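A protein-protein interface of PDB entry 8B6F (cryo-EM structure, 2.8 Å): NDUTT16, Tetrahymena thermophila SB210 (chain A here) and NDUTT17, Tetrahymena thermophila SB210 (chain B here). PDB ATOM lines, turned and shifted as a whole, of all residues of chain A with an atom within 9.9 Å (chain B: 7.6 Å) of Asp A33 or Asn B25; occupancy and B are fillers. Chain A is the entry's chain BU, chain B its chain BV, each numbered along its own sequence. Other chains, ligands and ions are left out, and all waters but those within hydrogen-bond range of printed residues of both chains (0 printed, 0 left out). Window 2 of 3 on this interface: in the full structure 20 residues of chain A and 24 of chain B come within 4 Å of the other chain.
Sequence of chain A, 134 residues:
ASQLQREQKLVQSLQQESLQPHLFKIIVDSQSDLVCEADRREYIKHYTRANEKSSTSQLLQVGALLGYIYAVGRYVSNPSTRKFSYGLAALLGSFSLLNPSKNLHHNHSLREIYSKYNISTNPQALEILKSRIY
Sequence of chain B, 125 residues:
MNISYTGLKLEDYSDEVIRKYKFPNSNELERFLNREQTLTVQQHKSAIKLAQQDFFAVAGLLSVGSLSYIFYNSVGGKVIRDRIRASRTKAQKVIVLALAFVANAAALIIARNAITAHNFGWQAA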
ATOM      1  N   ILE A  27      25.615   7.864  -7.526  1.00  0.00           N
ATOM      2  CA  ILE A  27      24.392   7.595  -6.774  1.00  0.00           C
ATOM      3  C   ILE A  27      24.227   6.095  -6.572  1.00  0.00           C
ATOM      4  O   ILE A  27      23.898   5.627  -5.476  1.00  0.00           O
ATOM      5  CB  ILE A  27      23.176   8.213  -7.487  1.00  0.00           C
ATOM      6  CG1 ILE A  27      23.322   9.735  -7.548  1.00  0.00           C
ATOM      7  CG2 ILE A  27      21.886   7.832  -6.767  1.00  0.00           C
ATOM      8  CD1 ILE A  27      22.242  10.432  -8.349  1.00  0.00           C
ATOM      9  N   VAL A  28      24.444   5.319  -7.634  1.00  0.00           N
ATOM     10  CA  VAL A  28      24.332   3.866  -7.541  1.00  0.00           C
ATOM     11  C   VAL A  28      25.273   3.328  -6.470  1.00  0.00           C
ATOM     12  O   VAL A  28      24.890   2.493  -5.644  1.00  0.00           O
ATOM     13  CB  VAL A  28      24.607   3.227  -8.915  1.00  0.00           C
ATOM     14  CG1 VAL A  28      25.028   1.768  -8.779  1.00  0.00           C
ATOM     15  CG2 VAL A  28      23.379   3.341  -9.799  1.00  0.00           C
ATOM     16  N   ASP A  29      26.519   3.806  -6.465  1.00  0.00           N
ATOM     17  CA  ASP A  29      27.472   3.374  -5.447  1.00  0.00           C
ATOM     18  C   ASP A  29      26.995   3.744  -4.049  1.00  0.00           C
ATOM     19  O   ASP A  29      27.123   2.949  -3.112  1.00  0.00           O
ATOM     20  CB  ASP A  29      28.844   3.985  -5.724  1.00  0.00           C
ATOM     21  CG  ASP A  29      29.449   3.491  -7.023  1.00  0.00           C
ATOM     22  OD1 ASP A  29      29.108   2.366  -7.445  1.00  0.00           O
ATOM     23  OD2 ASP A  29      30.267   4.223  -7.619  1.00  0.00           O
ATOM     24  N   SER A  30      26.442   4.946  -3.887  1.00  0.00           N
ATOM     25  CA  SER A  30      25.906   5.348  -2.594  1.00  0.00           C
ATOM     26  C   SER A  30      24.747   4.467  -2.148  1.00  0.00           C
ATOM     27  O   SER A  30      24.463   4.399  -0.948  1.00  0.00           O
ATOM     28  CB  SER A  30      25.445   6.801  -2.652  1.00  0.00           C
ATOM     29  OG  SER A  30      24.218   6.904  -3.351  1.00  0.00           O
ATOM     30  N   GLN A  31      24.064   3.808  -3.085  1.00  0.00           N
ATOM     31  CA  GLN A  31      22.973   2.884  -2.772  1.00  0.00           C
ATOM     32  C   GLN A  31      21.792   3.617  -2.147  1.00  0.00           C
ATOM     33  O   GLN A  31      21.149   3.118  -1.225  1.00  0.00           O
ATOM     34  CB  GLN A  31      23.440   1.759  -1.849  1.00  0.00           C
ATOM     35  CG  GLN A  31      24.483   0.853  -2.455  1.00  0.00           C
ATOM     36  CD  GLN A  31      24.839  -0.298  -1.538  1.00  0.00           C
ATOM     37  OE1 GLN A  31      24.310  -0.411  -0.434  1.00  0.00           O
ATOM     38  NE2 GLN A  31      25.738  -1.160  -1.994  1.00  0.00           N
ATOM     39  N   SER A  32      21.503   4.808  -2.658  1.00  0.00           N
ATOM     40  CA  SER A  32      20.381   5.582  -2.153  1.00  0.00           C
ATOM     41  C   SER A  32      19.074   4.838  -2.393  1.00  0.00           C
ATOM     42  O   SER A  32      18.907   4.150  -3.403  1.00  0.00           O
ATOM     43  CB  SER A  32      20.377   6.953  -2.817  1.00  0.00           C
ATOM     44  OG  SER A  32      21.626   7.573  -2.560  1.00  0.00           O
ATOM     45  N   ASP A  33      18.141   4.978  -1.450  1.00  0.00           N
ATOM     46  CA  ASP A  33      16.882   4.251  -1.541  1.00  0.00           C
ATOM     47  C   ASP A  33      16.046   4.668  -2.744  1.00  0.00           C
ATOM     48  O   ASP A  33      15.166   3.909  -3.162  1.00  0.00           O
ATOM     49  CB  ASP A  33      16.078   4.453  -0.256  1.00  0.00           C
ATOM     50  CG  ASP A  33      14.848   3.570  -0.193  1.00  0.00           C
ATOM     51  OD1 ASP A  33      14.991   2.375   0.141  1.00  0.00           O
ATOM     52  OD2 ASP A  33      13.741   4.068  -0.478  1.00  0.00           O
ATOM     53  N   LEU A  34      16.292   5.852  -3.310  1.00  0.00           N
ATOM     54  CA  LEU A  34      15.472   6.310  -4.427  1.00  0.00           C
ATOM     55  C   LEU A  34      15.648   5.418  -5.649  1.00  0.00           C
ATOM     56  O   LEU A  34      14.679   5.134  -6.364  1.00  0.00           O
ATOM     57  CB  LEU A  34      15.804   7.764  -4.768  1.00  0.00           C
ATOM     58  CG  LEU A  34      17.128   8.066  -5.470  1.00  0.00           C
ATOM     59  CD1 LEU A  34      16.974   8.047  -6.983  1.00  0.00           C
ATOM     60  CD2 LEU A  34      17.645   9.411  -5.017  1.00  0.00           C
ATOM     61  N   VAL A  35      16.871   4.968  -5.910  1.00  0.00           N
ATOM     62  CA  VAL A  35      17.143   4.133  -7.075  1.00  0.00           C
ATOM     63  C   VAL A  35      16.708   2.706  -6.778  1.00  0.00           C
ATOM     64  O   VAL A  35      17.134   2.107  -5.784  1.00  0.00           O
ATOM     65  CB  VAL A  35      18.631   4.194  -7.456  1.00  0.00           C
ATOM     66  CG1 VAL A  35      18.894   3.383  -8.715  1.00  0.00           C
ATOM     67  CG2 VAL A  35      19.074   5.636  -7.649  1.00  0.00           C
ATOM     68  N   CYS A  36      15.858   2.157  -7.641  1.00  0.00           N
ATOM     69  CA  CYS A  36      15.394   0.789  -7.469  1.00  0.00           C
ATOM     70  C   CYS A  36      16.548  -0.193  -7.630  1.00  0.00           C
ATOM     71  O   CYS A  36      17.533   0.077  -8.323  1.00  0.00           O
ATOM     72  CB  CYS A  36      14.294   0.472  -8.481  1.00  0.00           C
ATOM     73  SG  CYS A  36      13.647  -1.210  -8.374  1.00  0.00           S
ATOM     74  N   GLU A  37      16.420  -1.347  -6.974  1.00  0.00           N
ATOM     75  CA  GLU A  37      17.491  -2.337  -7.016  1.00  0.00           C
ATOM     76  C   GLU A  37      17.689  -2.885  -8.422  1.00  0.00           C
ATOM     77  O   GLU A  37      18.829  -3.080  -8.862  1.00  0.00           O
ATOM     78  CB  GLU A  37      17.194  -3.471  -6.036  1.00  0.00           C
ATOM     79  CG  GLU A  37      18.222  -4.591  -6.057  1.00  0.00           C
ATOM     80  CD  GLU A  37      19.630  -4.101  -5.785  1.00  0.00           C
ATOM     81  OE1 GLU A  37      19.777  -3.021  -5.175  1.00  0.00           O
ATOM     82  OE2 GLU A  37      20.590  -4.796  -6.182  1.00  0.00           O
ATOM     83  N   ALA A  38      16.598  -3.146  -9.145  1.00  0.00           N
ATOM     84  CA  ALA A  38      16.727  -3.681 -10.496  1.00  0.00           C
ATOM     85  C   ALA A  38      17.434  -2.688 -11.409  1.00  0.00           C
ATOM     86  O   ALA A  38      18.348  -3.054 -12.157  1.00  0.00           O
ATOM     87  CB  ALA A  38      15.348  -4.037 -11.052  1.00  0.00           C
ATOM     88  N   ASP A  39      17.020  -1.421 -11.359  1.00  0.00           N
ATOM     89  CA  ASP A  39      17.681  -0.398 -12.161  1.00  0.00           C
ATOM     90  C   ASP A  39      19.134  -0.241 -11.745  1.00  0.00           C
ATOM     91  O   ASP A  39      20.015  -0.039 -12.587  1.00  0.00           O
ATOM     92  CB  ASP A  39      16.940   0.932 -12.032  1.00  0.00           C
ATOM     93  CG  ASP A  39      15.523   0.864 -12.560  1.00  0.00           C
ATOM     94  OD1 ASP A  39      15.111  -0.219 -13.024  1.00  0.00           O
ATOM     95  OD2 ASP A  39      14.820   1.895 -12.517  1.00  0.00           O
ATOM     96  N   ARG A  40      19.401  -0.323 -10.441  1.00  0.00           N
ATOM     97  CA  ARG A  40      20.768  -0.219  -9.949  1.00  0.00           C
ATOM     98  C   ARG A  40      21.635  -1.339 -10.512  1.00  0.00           C
ATOM     99  O   ARG A  40      22.756  -1.102 -10.975  1.00  0.00           O
ATOM    100  CB  ARG A  40      20.756  -0.254  -8.421  1.00  0.00           C
ATOM    101  CG  ARG A  40      22.091   0.044  -7.789  1.00  0.00           C
ATOM    102  CD  ARG A  40      22.058  -0.122  -6.281  1.00  0.00           C
ATOM    103  NE  ARG A  40      23.392   0.018  -5.706  1.00  0.00           N
ATOM    104  CZ  ARG A  40      24.287  -0.958  -5.632  1.00  0.00           C
ATOM    105  NH1 ARG A  40      24.023  -2.176  -6.074  1.00  0.00           N
ATOM    106  NH2 ARG A  40      25.480  -0.703  -5.102  1.00  0.00           N
ATOM    107  N   TYR A 117      15.149   8.979 -13.563  1.00  0.00           N
ATOM    108  CA  TYR A 117      15.519   9.650 -12.322  1.00  0.00           C
ATOM    109  C   TYR A 117      15.901  11.107 -12.551  1.00  0.00           C
ATOM    110  O   TYR A 117      15.686  11.940 -11.666  1.00  0.00           O
ATOM    111  CB  TYR A 117      16.667   8.901 -11.648  1.00  0.00           C
ATOM    112  CG  TYR A 117      16.281   7.515 -11.195  1.00  0.00           C
ATOM    113  CD1 TYR A 117      15.568   7.322 -10.020  1.00  0.00           C
ATOM    114  CD2 TYR A 117      16.623   6.399 -11.946  1.00  0.00           C
ATOM    115  CE1 TYR A 117      15.209   6.057  -9.603  1.00  0.00           C
ATOM    116  CE2 TYR A 117      16.266   5.130 -11.538  1.00  0.00           C
ATOM    117  CZ  TYR A 117      15.559   4.966 -10.366  1.00  0.00           C
ATOM    118  OH  TYR A 117      15.203   3.705  -9.951  1.00  0.00           O
ATOM    119  N   ASN A 122      16.917  17.461  -9.206  1.00  0.00           N
ATOM    120  CA  ASN A 122      16.349  16.476  -8.285  1.00  0.00           C
ATOM    121  C   ASN A 122      16.926  16.713  -6.897  1.00  0.00           C
ATOM    122  O   ASN A 122      18.132  16.482  -6.686  1.00  0.00           O
ATOM    123  CB  ASN A 122      16.649  15.054  -8.758  1.00  0.00           C
ATOM    124  CG  ASN A 122      15.984  14.000  -7.897  1.00  0.00           C
ATOM    125  OD1 ASN A 122      15.074  14.297  -7.124  1.00  0.00           O
ATOM    126  ND2 ASN A 122      16.435  12.760  -8.027  1.00  0.00           N
ATOM    127  N   GLN A 124      16.780  15.096  -4.063  1.00  0.00           N
ATOM    128  CA  GLN A 124      17.374  13.916  -3.445  1.00  0.00           C
ATOM    129  C   GLN A 124      18.712  13.576  -4.087  1.00  0.00           C
ATOM    130  O   GLN A 124      19.677  13.245  -3.387  1.00  0.00           O
ATOM    131  CB  GLN A 124      16.411  12.733  -3.538  1.00  0.00           C
ATOM    132  CG  GLN A 124      15.080  12.979  -2.845  1.00  0.00           C
ATOM    133  CD  GLN A 124      14.139  11.798  -2.955  1.00  0.00           C
ATOM    134  OE1 GLN A 124      14.499  10.749  -3.488  1.00  0.00           O
ATOM    135  NE2 GLN A 124      12.921  11.964  -2.450  1.00  0.00           N
ATOM    136  N   ALA A 125      18.791  13.648  -5.416  1.00  0.00           N
ATOM    137  CA  ALA A 125      20.059  13.399  -6.092  1.00  0.00           C
ATOM    138  C   ALA A 125      21.108  14.428  -5.689  1.00  0.00           C
ATOM    139  O   ALA A 125      22.269  14.080  -5.450  1.00  0.00           O
ATOM    140  CB  ALA A 125      19.857  13.407  -7.606  1.00  0.00           C
ATOM    141  N   ILE A 128      22.392  13.551  -2.271  1.00  0.00           N
ATOM    142  CA  ILE A 128      23.290  12.402  -2.344  1.00  0.00           C
ATOM    143  C   ILE A 128      24.650  12.820  -2.887  1.00  0.00           C
ATOM    144  O   ILE A 128      25.694  12.423  -2.359  1.00  0.00           O
ATOM    145  CB  ILE A 128      22.648  11.314  -3.221  1.00  0.00           C
ATOM    146  CG1 ILE A 128      21.347  10.825  -2.587  1.00  0.00           C
ATOM    147  CG2 ILE A 128      23.599  10.148  -3.408  1.00  0.00           C
ATOM    148  CD1 ILE A 128      20.378  10.236  -3.583  1.00  0.00           C
ATOM    149  N   ARG A 132      29.266  13.277  -1.762  1.00  0.00           N
ATOM    150  CA  ARG A 132      30.171  12.423  -2.529  1.00  0.00           C
ATOM    151  C   ARG A 132      30.610  13.174  -3.783  1.00  0.00           C
ATOM    152  O   ARG A 132      29.899  13.176  -4.793  1.00  0.00           O
ATOM    153  CB  ARG A 132      29.496  11.103  -2.888  1.00  0.00           C
ATOM    154  CG  ARG A 132      28.978  10.331  -1.689  1.00  0.00           C
ATOM    155  CD  ARG A 132      27.936   9.310  -2.100  1.00  0.00           C
ATOM    156  NE  ARG A 132      27.440   8.557  -0.955  1.00  0.00           N
ATOM    157  CZ  ARG A 132      26.474   8.968  -0.146  1.00  0.00           C
ATOM    158  NH1 ARG A 132      25.877  10.135  -0.318  1.00  0.00           N
ATOM    159  NH2 ARG A 132      26.099   8.189   0.864  1.00  0.00           N
ATOM    160  N   LYS B  22      10.807  -7.116  11.811  1.00  0.00           N
ATOM    161  CA  LYS B  22      10.178  -6.619  10.597  1.00  0.00           C
ATOM    162  C   LYS B  22      11.146  -6.707   9.422  1.00  0.00           C
ATOM    163  O   LYS B  22      12.356  -6.540   9.576  1.00  0.00           O
ATOM    164  CB  LYS B  22       9.709  -5.173  10.776  1.00  0.00           C
ATOM    165  CG  LYS B  22      10.829  -4.143  10.731  1.00  0.00           C
ATOM    166  CD  LYS B  22      10.322  -2.761  11.109  1.00  0.00           C
ATOM    167  CE  LYS B  22      11.443  -1.739  11.087  1.00  0.00           C
ATOM    168  NZ  LYS B  22      12.081  -1.637   9.745  1.00  0.00           N
ATOM    169  N   PHE B  23      10.594  -6.980   8.244  1.00  0.00           N
ATOM    170  CA  PHE B  23      11.415  -7.054   7.048  1.00  0.00           C
ATOM    171  C   PHE B  23      12.028  -5.687   6.753  1.00  0.00           C
ATOM    172  O   PHE B  23      11.360  -4.659   6.914  1.00  0.00           O
ATOM    173  CB  PHE B  23      10.579  -7.510   5.849  1.00  0.00           C
ATOM    174  CG  PHE B  23      10.585  -8.997   5.618  1.00  0.00           C
ATOM    175  CD1 PHE B  23      11.764  -9.724   5.661  1.00  0.00           C
ATOM    176  CD2 PHE B  23       9.406  -9.665   5.339  1.00  0.00           C
ATOM    177  CE1 PHE B  23      11.763 -11.087   5.438  1.00  0.00           C
ATOM    178  CE2 PHE B  23       9.400 -11.028   5.116  1.00  0.00           C
ATOM    179  CZ  PHE B  23      10.580 -11.738   5.166  1.00  0.00           C
ATOM    180  N   PRO B  24      13.289  -5.631   6.319  1.00  0.00           N
ATOM    181  CA  PRO B  24      13.872  -4.340   5.930  1.00  0.00           C
ATOM    182  C   PRO B  24      13.357  -3.851   4.587  1.00  0.00           C
ATOM    183  O   PRO B  24      12.452  -4.452   4.000  1.00  0.00           O
ATOM    184  CB  PRO B  24      15.376  -4.637   5.888  1.00  0.00           C
ATOM    185  CG  PRO B  24      15.461  -6.079   5.576  1.00  0.00           C
ATOM    186  CD  PRO B  24      14.274  -6.725   6.236  1.00  0.00           C
ATOM    187  N   ASN B  25      13.924  -2.748   4.104  1.00  0.00           N
ATOM    188  CA  ASN B  25      13.520  -2.174   2.829  1.00  0.00           C
ATOM    189  C   ASN B  25      13.587  -3.220   1.723  1.00  0.00           C
ATOM    190  O   ASN B  25      14.337  -4.196   1.804  1.00  0.00           O
ATOM    191  CB  ASN B  25      14.414  -0.980   2.486  1.00  0.00           C
ATOM    192  CG  ASN B  25      14.086  -0.373   1.141  1.00  0.00           C
ATOM    193  OD1 ASN B  25      14.642  -0.769   0.116  1.00  0.00           O
ATOM    194  ND2 ASN B  25      13.178   0.596   1.133  1.00  0.00           N
ATOM    195  N   SER B  26      12.787  -3.009   0.675  1.00  0.00           N
ATOM    196  CA  SER B  26      12.761  -3.955  -0.435  1.00  0.00           C
ATOM    197  C   SER B  26      14.117  -4.029  -1.125  1.00  0.00           C
ATOM    198  O   SER B  26      14.563  -5.111  -1.520  1.00  0.00           O
ATOM    199  CB  SER B  26      11.675  -3.560  -1.435  1.00  0.00           C
ATOM    200  OG  SER B  26      11.627  -4.474  -2.516  1.00  0.00           O
ATOM    201  N   ASN B  27      14.786  -2.886  -1.282  1.00  0.00           N
ATOM    202  CA  ASN B  27      16.111  -2.887  -1.894  1.00  0.00           C
ATOM    203  C   ASN B  27      17.096  -3.686  -1.055  1.00  0.00           C
ATOM    204  O   ASN B  27      17.892  -4.466  -1.591  1.00  0.00           O
ATOM    205  CB  ASN B  27      16.607  -1.454  -2.085  1.00  0.00           C
ATOM    206  CG  ASN B  27      15.632  -0.598  -2.865  1.00  0.00           C
ATOM    207  OD1 ASN B  27      14.449  -0.921  -2.966  1.00  0.00           O
ATOM    208  ND2 ASN B  27      16.124   0.498  -3.427  1.00  0.00           N
ATOM    209  N   GLU B  28      17.054  -3.510   0.267  1.00  0.00           N
ATOM    210  CA  GLU B  28      17.931  -4.276   1.146  1.00  0.00           C
ATOM    211  C   GLU B  28      17.638  -5.768   1.047  1.00  0.00           C
ATOM    212  O   GLU B  28      18.562  -6.589   1.009  1.00  0.00           O
ATOM    213  CB  GLU B  28      17.771  -3.799   2.588  1.00  0.00           C
ATOM    214  CG  GLU B  28      18.066  -2.322   2.792  1.00  0.00           C
ATOM    215  CD  GLU B  28      19.530  -1.984   2.604  1.00  0.00           C
ATOM    216  OE1 GLU B  28      20.340  -2.919   2.433  1.00  0.00           O
ATOM    217  OE2 GLU B  28      19.873  -0.785   2.630  1.00  0.00           O
ATOM    218  N   LEU B  29      16.357  -6.140   1.011  1.00  0.00           N
ATOM    219  CA  LEU B  29      16.004  -7.547   0.871  1.00  0.00           C
ATOM    220  C   LEU B  29      16.535  -8.118  -0.436  1.00  0.00           C
ATOM    221  O   LEU B  29      17.071  -9.232  -0.463  1.00  0.00           O
ATOM    222  CB  LEU B  29      14.487  -7.721   0.950  1.00  0.00           C
ATOM    223  CG  LEU B  29      13.862  -7.709   2.346  1.00  0.00           C
ATOM    224  CD1 LEU B  29      12.350  -7.722   2.245  1.00  0.00           C
ATOM    225  CD2 LEU B  29      14.344  -8.893   3.168  1.00  0.00           C
ATOM    226  N   GLU B  30      16.398  -7.371  -1.531  1.00  0.00           N
ATOM    227  CA  GLU B  30      16.892  -7.853  -2.816  1.00  0.00           C
ATOM    228  C   GLU B  30      18.406  -8.019  -2.801  1.00  0.00           C
ATOM    229  O   GLU B  30      18.931  -9.017  -3.310  1.00  0.00           O
ATOM    230  CB  GLU B  30      16.469  -6.896  -3.929  1.00  0.00           C
ATOM    231  CG  GLU B  30      14.981  -6.922  -4.234  1.00  0.00           C
ATOM    232  CD  GLU B  30      14.529  -8.246  -4.817  1.00  0.00           C
ATOM    233  OE1 GLU B  30      15.396  -9.039  -5.239  1.00  0.00           O
ATOM    234  OE2 GLU B  30      13.306  -8.495  -4.850  1.00  0.00           O
ATOM    235  N   ARG B  31      19.128  -7.054  -2.230  1.00  0.00           N
ATOM    236  CA  ARG B  31      20.581  -7.175  -2.156  1.00  0.00           C
ATOM    237  C   ARG B  31      20.986  -8.399  -1.346  1.00  0.00           C
ATOM    238  O   ARG B  31      21.878  -9.156  -1.744  1.00  0.00           O
ATOM    239  CB  ARG B  31      21.180  -5.911  -1.540  1.00  0.00           C
ATOM    240  CG  ARG B  31      21.048  -4.674  -2.403  1.00  0.00           C
ATOM    241  CD  ARG B  31      21.815  -3.508  -1.805  1.00  0.00           C
ATOM    242  NE  ARG B  31      21.449  -2.244  -2.434  1.00  0.00           N
ATOM    243  CZ  ARG B  31      20.501  -1.427  -1.993  1.00  0.00           C
ATOM    244  NH1 ARG B  31      19.799  -1.701  -0.908  1.00  0.00           N
ATOM    245  NH2 ARG B  31      20.253  -0.304  -2.660  1.00  0.00           N
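The guanidinium group (NH2) of Arg A40 lies close to the side-chain amide nitrogen (NE2) of Gln A31 (3.2 Å).
N of Asn B27 sits at hydrogen-bond distance from OD1 of Asn B25 (2.5 Å).
The backbone carbonyl oxygen (O) of Asn B27 lies close to the guanidinium group (NH1) of Arg B31.
OE1 of Glu B28 lies within salt-bridge range of NH1 of Arg B31.
Asp A33 touches two residues of chain B.
Asn A122 touches none of the printed residues of chain B.
Asn B25 touches just one residue of chain A: Asp A33 (2.7 Å).
Ser B26 touches none of the printed residues of chain A.
Of the printed residues of chain A, Asn B27 touches Asp A33 (3.6 Å) and Val A35 (3.0 Å).
Of the printed residues of chain A, Glu B30 touches Glu A37 (3.6 Å).
Of the printed residues of chain A, Arg B31 touches Gln A31 and Glu A37.
The nearest residue of chain B that does not touch Asp A33 is Arg B31 (5.8 Å).
Of the 10 printed residues of chain B, 4 touch a printed residue of chain A.
Printed residues of chain B that touch a printed residue of chain A: Asn B25, Asn B27, Glu B30 and Arg B31.
Of the 20 printed residues of chain A, 4 touch a printed residue of chain B.
Printed residues of chain A that touch a printed residue of chain B: Gln A31, Asp A33, Val A35 and Glu A37.
Along chain A the printed residues that touch a printed residue of chain B span positions 31 to 37.
Among the printed residues, 6 pairs touch across the chains.
Among the printed residues, Asp or Glu carboxylates within 4 Å of a Lys or Arg side-chain nitrogen of the other chain: Glu A37 with Arg B31.
Arg B31 touches Gln A31 (NH2 to O, 3.8 Å).
Asn B27 touches Asp A33.
Glu B30 touches Glu A37.
OD1 of Asp A33 is in hydrogen-bond range of ND2 of Asn B25, at 2.7 Å.
The side-chain amide nitrogen (ND2) of Asn B27 is in hydrogen-bond range of the backbone carbonyl oxygen (O) of Val A35 (3.0 Å).
OE1 of Glu A37 lies within salt-bridge range of NE of Arg B31, 3.3 Å away.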
